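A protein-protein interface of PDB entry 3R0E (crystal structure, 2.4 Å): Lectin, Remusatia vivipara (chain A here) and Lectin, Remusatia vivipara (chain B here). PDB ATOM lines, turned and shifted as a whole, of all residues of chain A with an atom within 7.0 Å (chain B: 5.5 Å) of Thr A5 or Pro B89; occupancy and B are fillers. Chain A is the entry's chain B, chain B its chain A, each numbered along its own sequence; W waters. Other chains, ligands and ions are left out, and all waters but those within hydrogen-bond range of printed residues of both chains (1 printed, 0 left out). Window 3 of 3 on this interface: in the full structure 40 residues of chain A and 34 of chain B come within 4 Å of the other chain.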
ATOM      1  N   ILE A   2     -22.312  13.034 -11.206  1.00  0.00           N
ATOM      2  CA  ILE A   2     -22.199  14.389 -10.680  1.00  0.00           C
ATOM      3  C   ILE A   2     -21.652  14.326  -9.247  1.00  0.00           C
ATOM      4  O   ILE A   2     -22.098  13.484  -8.451  1.00  0.00           O
ATOM      5  CB  ILE A   2     -23.584  15.104 -10.749  1.00  0.00           C
ATOM      6  CG1 ILE A   2     -24.058  15.187 -12.214  1.00  0.00           C
ATOM      7  CG2 ILE A   2     -23.542  16.489 -10.084  1.00  0.00           C
ATOM      8  CD1 ILE A   2     -25.582  15.255 -12.400  1.00  0.00           C
ATOM      9  N   PRO A   3     -20.664  15.192  -8.922  1.00  0.00           N
ATOM     10  CA  PRO A   3     -20.175  15.290  -7.535  1.00  0.00           C
ATOM     11  C   PRO A   3     -21.303  15.629  -6.567  1.00  0.00           C
ATOM     12  O   PRO A   3     -22.225  16.383  -6.915  1.00  0.00           O
ATOM     13  CB  PRO A   3     -19.159  16.441  -7.586  1.00  0.00           C
ATOM     14  CG  PRO A   3     -18.693  16.475  -9.010  1.00  0.00           C
ATOM     15  CD  PRO A   3     -19.887  16.043  -9.846  1.00  0.00           C
ATOM     16  N   PHE A   4     -21.236  15.047  -5.375  1.00  0.00           N
ATOM     17  CA  PHE A   4     -22.210  15.320  -4.327  1.00  0.00           C
ATOM     18  C   PHE A   4     -21.879  16.593  -3.562  1.00  0.00           C
ATOM     19  O   PHE A   4     -20.709  16.915  -3.344  1.00  0.00           O
ATOM     20  CB  PHE A   4     -22.367  14.118  -3.374  1.00  0.00           C
ATOM     21  CG  PHE A   4     -23.348  13.084  -3.867  1.00  0.00           C
ATOM     22  CD1 PHE A   4     -24.716  13.218  -3.602  1.00  0.00           C
ATOM     23  CD2 PHE A   4     -22.915  11.992  -4.629  1.00  0.00           C
ATOM     24  CE1 PHE A   4     -25.637  12.268  -4.075  1.00  0.00           C
ATOM     25  CE2 PHE A   4     -23.828  11.041  -5.111  1.00  0.00           C
ATOM     26  CZ  PHE A   4     -25.191  11.182  -4.830  1.00  0.00           C
ATOM     27  N   THR A   5     -22.931  17.332  -3.221  1.00  0.00           N
ATOM     28  CA  THR A   5     -22.883  18.427  -2.248  1.00  0.00           C
ATOM     29  C   THR A   5     -23.906  18.079  -1.169  1.00  0.00           C
ATOM     30  O   THR A   5     -24.976  17.534  -1.470  1.00  0.00           O
ATOM     31  CB  THR A   5     -23.235  19.798  -2.871  1.00  0.00           C
ATOM     32  OG1 THR A   5     -22.433  20.032  -4.032  1.00  0.00           O
ATOM     33  CG2 THR A   5     -22.999  20.931  -1.855  1.00  0.00           C
ATOM     34  N   ASN A   6     -23.566  18.412   0.076  1.00  0.00           N
ATOM     35  CA  ASN A   6     -24.300  17.964   1.262  1.00  0.00           C
ATOM     36  C   ASN A   6     -25.788  18.313   1.305  1.00  0.00           C
ATOM     37  O   ASN A   6     -26.579  17.545   1.830  1.00  0.00           O
ATOM     38  CB  ASN A   6     -23.618  18.505   2.519  1.00  0.00           C
ATOM     39  CG  ASN A   6     -23.614  20.031   2.563  1.00  0.00           C
ATOM     40  OD1 ASN A   6     -22.959  20.693   1.737  1.00  0.00           O
ATOM     41  ND2 ASN A   6     -24.361  20.601   3.520  1.00  0.00           N
ATOM     42  N   ASN A   7     -26.166  19.474   0.778  1.00  0.00           N
ATOM     43  CA  ASN A   7     -27.554  19.925   0.861  1.00  0.00           C
ATOM     44  C   ASN A   7     -28.296  19.899  -0.476  1.00  0.00           C
ATOM     45  O   ASN A   7     -29.408  20.426  -0.579  1.00  0.00           O
ATOM     46  CB  ASN A   7     -27.625  21.327   1.482  1.00  0.00           C
ATOM     47  CG  ASN A   7     -26.966  22.382   0.621  1.00  0.00           C
ATOM     48  OD1 ASN A   7     -26.047  22.093  -0.145  1.00  0.00           O
ATOM     49  ND2 ASN A   7     -27.424  23.612   0.749  1.00  0.00           N
ATOM     50  N   LEU A   8     -27.684  19.290  -1.489  1.00  0.00           N
ATOM     51  CA  LEU A   8     -28.235  19.324  -2.843  1.00  0.00           C
ATOM     52  C   LEU A   8     -28.404  17.938  -3.449  1.00  0.00           C
ATOM     53  O   LEU A   8     -27.587  17.045  -3.211  1.00  0.00           O
ATOM     54  CB  LEU A   8     -27.340  20.152  -3.770  1.00  0.00           C
ATOM     55  CG  LEU A   8     -26.887  21.569  -3.404  1.00  0.00           C
ATOM     56  CD1 LEU A   8     -25.809  22.050  -4.386  1.00  0.00           C
ATOM     57  CD2 LEU A   8     -28.048  22.544  -3.353  1.00  0.00           C
ATOM     58  N   LEU A   9     -29.453  17.772  -4.253  1.00  0.00           N
ATOM     59  CA  LEU A   9     -29.578  16.590  -5.105  1.00  0.00           C
ATOM     60  C   LEU A   9     -30.020  17.014  -6.499  1.00  0.00           C
ATOM     61  O   LEU A   9     -31.126  17.521  -6.678  1.00  0.00           O
ATOM     62  CB  LEU A   9     -30.549  15.578  -4.499  1.00  0.00           C
ATOM     63  CG  LEU A   9     -30.561  14.150  -5.037  1.00  0.00           C
ATOM     64  CD1 LEU A   9     -29.307  13.401  -4.613  1.00  0.00           C
ATOM     65  CD2 LEU A   9     -31.809  13.438  -4.528  1.00  0.00           C
ATOM     66  N   PHE A  10     -29.141  16.831  -7.477  1.00  0.00           N
ATOM     67  CA  PHE A  10     -29.431  17.216  -8.846  1.00  0.00           C
ATOM     68  C   PHE A  10     -30.025  16.035  -9.579  1.00  0.00           C
ATOM     69  O   PHE A  10     -29.835  14.881  -9.170  1.00  0.00           O
ATOM     70  CB  PHE A  10     -28.166  17.679  -9.576  1.00  0.00           C
ATOM     71  CG  PHE A  10     -27.582  18.949  -9.031  1.00  0.00           C
ATOM     72  CD1 PHE A  10     -28.035  20.185  -9.479  1.00  0.00           C
ATOM     73  CD2 PHE A  10     -26.584  18.912  -8.059  1.00  0.00           C
ATOM     74  CE1 PHE A  10     -27.506  21.358  -8.963  1.00  0.00           C
ATOM     75  CE2 PHE A  10     -26.051  20.084  -7.546  1.00  0.00           C
ATOM     76  CZ  PHE A  10     -26.499  21.306  -8.001  1.00  0.00           C
ATOM     77  N   GLN A  13     -28.877  12.191  -9.766  1.00  0.00           N
ATOM     78  CA  GLN A  13     -28.192  11.767  -8.550  1.00  0.00           C
ATOM     79  C   GLN A  13     -29.095  10.864  -7.712  1.00  0.00           C
ATOM     80  O   GLN A  13     -30.330  10.960  -7.778  1.00  0.00           O
ATOM     81  CB  GLN A  13     -27.697  12.960  -7.728  1.00  0.00           C
ATOM     82  CG  GLN A  13     -26.601  13.746  -8.412  1.00  0.00           C
ATOM     83  CD  GLN A  13     -25.894  14.705  -7.482  1.00  0.00           C
ATOM     84  OE1 GLN A  13     -26.518  15.572  -6.857  1.00  0.00           O
ATOM     85  NE2 GLN A  13     -24.579  14.562  -7.388  1.00  0.00           N
ATOM     86  N   ARG A  20     -27.943  10.806   2.926  1.00  0.00           N
ATOM     87  CA  ARG A  20     -28.743  11.918   3.408  1.00  0.00           C
ATOM     88  C   ARG A  20     -28.342  13.239   2.779  1.00  0.00           C
ATOM     89  O   ARG A  20     -27.213  13.396   2.298  1.00  0.00           O
ATOM     90  CB  ARG A  20     -28.606  12.034   4.935  1.00  0.00           C
ATOM     91  CG  ARG A  20     -27.162  12.176   5.401  1.00  0.00           C
ATOM     92  CD  ARG A  20     -27.010  12.245   6.915  1.00  0.00           C
ATOM     93  NE  ARG A  20     -27.802  11.233   7.607  1.00  0.00           N
ATOM     94  CZ  ARG A  20     -27.470   9.951   7.690  1.00  0.00           C
ATOM     95  NH1 ARG A  20     -26.350   9.517   7.115  1.00  0.00           N
ATOM     96  NH2 ARG A  20     -28.255   9.101   8.335  1.00  0.00           N
ATOM     97  N   LEU A  21     -29.283  14.181   2.777  1.00  0.00           N
ATOM     98  CA  LEU A  21     -28.946  15.595   2.627  1.00  0.00           C
ATOM     99  C   LEU A  21     -28.844  16.204   4.019  1.00  0.00           C
ATOM    100  O   LEU A  21     -29.577  15.816   4.935  1.00  0.00           O
ATOM    101  CB  LEU A  21     -29.979  16.347   1.774  1.00  0.00           C
ATOM    102  CG  LEU A  21     -30.211  15.904   0.319  1.00  0.00           C
ATOM    103  CD1 LEU A  21     -31.076  16.915  -0.444  1.00  0.00           C
ATOM    104  CD2 LEU A  21     -28.902  15.663  -0.435  1.00  0.00           C
ATOM    105  N   THR A  22     -27.937  17.159   4.169  1.00  0.00           N
ATOM    106  CA  THR A  22     -27.677  17.797   5.446  1.00  0.00           C
ATOM    107  C   THR A  22     -27.754  19.313   5.304  1.00  0.00           C
ATOM    108  O   THR A  22     -27.162  19.890   4.393  1.00  0.00           O
ATOM    109  CB  THR A  22     -26.270  17.410   5.984  1.00  0.00           C
ATOM    110  OG1 THR A  22     -26.195  15.993   6.144  1.00  0.00           O
ATOM    111  CG2 THR A  22     -26.009  18.052   7.324  1.00  0.00           C
ATOM    112  N   ASN B   4     -24.457  27.805  -0.294  1.00  0.00           N
ATOM    113  CA  ASN B   4     -24.164  27.611  -1.712  1.00  0.00           C
ATOM    114  C   ASN B   4     -25.342  27.986  -2.617  1.00  0.00           C
ATOM    115  O   ASN B   4     -25.352  27.644  -3.798  1.00  0.00           O
ATOM    116  CB  ASN B   4     -23.729  26.162  -1.975  1.00  0.00           C
ATOM    117  CG  ASN B   4     -24.733  25.158  -1.472  1.00  0.00           C
ATOM    118  OD1 ASN B   4     -25.880  25.500  -1.176  1.00  0.00           O
ATOM    119  ND2 ASN B   4     -24.316  23.910  -1.368  1.00  0.00           N
ATOM    120  N   ASN B  20     -19.307  26.715  -2.809  1.00  0.00           N
ATOM    121  CA  ASN B  20     -19.380  25.273  -2.984  1.00  0.00           C
ATOM    122  C   ASN B  20     -18.000  24.792  -3.395  1.00  0.00           C
ATOM    123  O   ASN B  20     -17.544  25.074  -4.504  1.00  0.00           O
ATOM    124  CB  ASN B  20     -20.419  24.890  -4.038  1.00  0.00           C
ATOM    125  CG  ASN B  20     -20.834  23.430  -3.950  1.00  0.00           C
ATOM    126  OD1 ASN B  20     -20.043  22.560  -3.575  1.00  0.00           O
ATOM    127  ND2 ASN B  20     -22.080  23.152  -4.308  1.00  0.00           N
ATOM    128  N   PHE B  23     -15.262  26.892  -5.415  1.00  0.00           N
ATOM    129  CA  PHE B  23     -15.949  27.980  -6.090  1.00  0.00           C
ATOM    130  C   PHE B  23     -16.675  28.864  -5.099  1.00  0.00           C
ATOM    131  O   PHE B  23     -17.409  28.389  -4.236  1.00  0.00           O
ATOM    132  CB  PHE B  23     -16.901  27.443  -7.146  1.00  0.00           C
ATOM    133  CG  PHE B  23     -16.266  26.468  -8.075  1.00  0.00           C
ATOM    134  CD1 PHE B  23     -15.438  26.911  -9.106  1.00  0.00           C
ATOM    135  CD2 PHE B  23     -16.482  25.100  -7.919  1.00  0.00           C
ATOM    136  CE1 PHE B  23     -14.842  26.009  -9.978  1.00  0.00           C
ATOM    137  CE2 PHE B  23     -15.889  24.182  -8.785  1.00  0.00           C
ATOM    138  CZ  PHE B  23     -15.064  24.639  -9.817  1.00  0.00           C
ATOM    139  N   VAL B  87     -24.574  27.660  -6.584  1.00  0.00           N
ATOM    140  CA  VAL B  87     -23.207  27.389  -6.976  1.00  0.00           C
ATOM    141  C   VAL B  87     -23.114  25.879  -7.122  1.00  0.00           C
ATOM    142  O   VAL B  87     -23.029  25.151  -6.134  1.00  0.00           O
ATOM    143  CB  VAL B  87     -22.200  27.944  -5.939  1.00  0.00           C
ATOM    144  CG1 VAL B  87     -20.754  27.728  -6.400  1.00  0.00           C
ATOM    145  CG2 VAL B  87     -22.453  29.426  -5.727  1.00  0.00           C
ATOM    146  N   HIS B  88     -23.223  25.417  -8.362  1.00  0.00           N
ATOM    147  CA  HIS B  88     -23.096  24.007  -8.702  1.00  0.00           C
ATOM    148  C   HIS B  88     -21.639  23.553  -8.474  1.00  0.00           C
ATOM    149  O   HIS B  88     -20.704  24.301  -8.775  1.00  0.00           O
ATOM    150  CB  HIS B  88     -23.484  23.836 -10.172  1.00  0.00           C
ATOM    151  CG  HIS B  88     -23.581  22.413 -10.624  1.00  0.00           C
ATOM    152  ND1 HIS B  88     -24.785  21.799 -10.891  1.00  0.00           N
ATOM    153  CD2 HIS B  88     -22.625  21.487 -10.866  1.00  0.00           C
ATOM    154  CE1 HIS B  88     -24.567  20.554 -11.270  1.00  0.00           C
ATOM    155  NE2 HIS B  88     -23.264  20.340 -11.268  1.00  0.00           N
ATOM    156  N   PRO B  89     -21.437  22.328  -7.950  1.00  0.00           N
ATOM    157  CA  PRO B  89     -20.063  21.858  -7.665  1.00  0.00           C
ATOM    158  C   PRO B  89     -19.155  21.711  -8.888  1.00  0.00           C
ATOM    159  O   PRO B  89     -17.954  21.555  -8.723  1.00  0.00           O
ATOM    160  CB  PRO B  89     -20.283  20.497  -7.002  1.00  0.00           C
ATOM    161  CG  PRO B  89     -21.590  20.029  -7.555  1.00  0.00           C
ATOM    162  CD  PRO B  89     -22.435  21.294  -7.619  1.00  0.00           C
ATOM    163  N   ASP B  90     -19.716  21.748 -10.094  1.00  0.00           N
ATOM    164  CA  ASP B  90     -18.909  21.783 -11.323  1.00  0.00           C
ATOM    165  C   ASP B  90     -18.445  23.203 -11.661  1.00  0.00           C
ATOM    166  O   ASP B  90     -17.802  23.435 -12.686  1.00  0.00           O
ATOM    167  CB  ASP B  90     -19.652  21.143 -12.512  1.00  0.00           C
ATOM    168  CG  ASP B  90     -19.574  19.604 -12.510  1.00  0.00           C
ATOM    169  OD1 ASP B  90     -18.638  19.041 -11.884  1.00  0.00           O
ATOM    170  OD2 ASP B  90     -20.444  18.947 -13.149  1.00  0.00           O
ATOM    171  N   GLY B  91     -18.775  24.150 -10.791  1.00  0.00           N
ATOM    172  CA  GLY B  91     -18.263  25.518 -10.889  1.00  0.00           C
ATOM    173  C   GLY B  91     -19.055  26.451 -11.777  1.00  0.00           C
ATOM    174  O   GLY B  91     -18.490  27.352 -12.395  1.00  0.00           O
HETATM  175  O   HOH W   1     -19.105  19.948  -3.436  1.00  0.00           O
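Water W1 lies within hydrogen-bond range of the side-chain amide oxygen of Asn B20, the side-chain hydroxyl of Thr A5 and the backbone carbonyl oxygen of Phe A4.
The backbone NH of Val B87 lies within hydrogen-bond range of the backbone carbonyl oxygen of Asn B4. The side-chain amide nitrogen of Asn B20 lies within hydrogen-bond range of the backbone carbonyl oxygen of Val B87, at 2.9 Å. The backbone NH (N) of Phe A10 is in hydrogen-bond range of the side-chain amide oxygen (OE1) of Gln A13, 3.0 Å away. O of Pro A3 sits at hydrogen-bond distance from NE2 of Gln A13, at 3.0 Å.
The side-chain amide nitrogen of Asn B20 is in hydrogen-bond range of the side-chain hydroxyl of Thr A5 (3.2 Å). The side-chain amide nitrogen (ND2) of Asn B4 lies within hydrogen-bond range of the side-chain amide oxygen (OD1) of Asn A7, at 2.8 Å.
Of chain B, only Asn B4 (3.3 Å), Asn B20 (3.2 Å) and Pro B89 (3.6 Å) come within 4 Å of Thr A5. Of chain A, only Pro A3, Thr A5 and Phe A10 come within 4 Å of Pro B89. Of the printed residues of chain B, Pro A3 touches Pro B89 and Asp B90. Of the printed residues of chain A, His B88 touches Phe A10. Of the printed residues of chain A, Asn B20 touches Thr A5 (3.2 Å) and Leu A8 (3.9 Å). The nearest printed residue of chain B that does not touch Thr A5 is Val B87 (5.6 Å). The nearest residue of chain A that does not touch Pro B89 is Leu A8 (4.7 Å).
Pro A3 touches Pro B89 (O to CG, 3.8 Å). OD1 of Asp B90 touches CD of Pro A3, at 3.8 Å. CG2 of Thr A5 touches ND2 of Asn B4, 3.3 Å away. OG1 of Thr A5 touches CG of Pro B89, 3.6 Å away. Leu A8 touches Asn B4 (CD1 to ND2, 3.8 Å). Asn B20 touches Leu A8 (ND2 to CD1, 3.9 Å). ND1 of His B88 touches CE1 of Phe A10, 3.4 Å away. Phe A10 touches Pro B89 (CE2 to CD, 3.8 Å).
Of the 8 printed residues of chain B, 5 touch a printed residue of chain A. Printed residues of chain B that touch a printed residue of chain A: Asn B4, Asn B20, His B88, Pro B89 and Asp B90. Hydrophobic or aromatic side chains of chain A within 4 Å of the printed part of chain B: Pro A3, Leu A8 and Phe A10. Among the printed residues, 10 pairs touch across the chains. Among the printed residues, no Asp or Glu carboxylate lies within 4 Å of a Lys or Arg side-chain nitrogen of the other chain.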
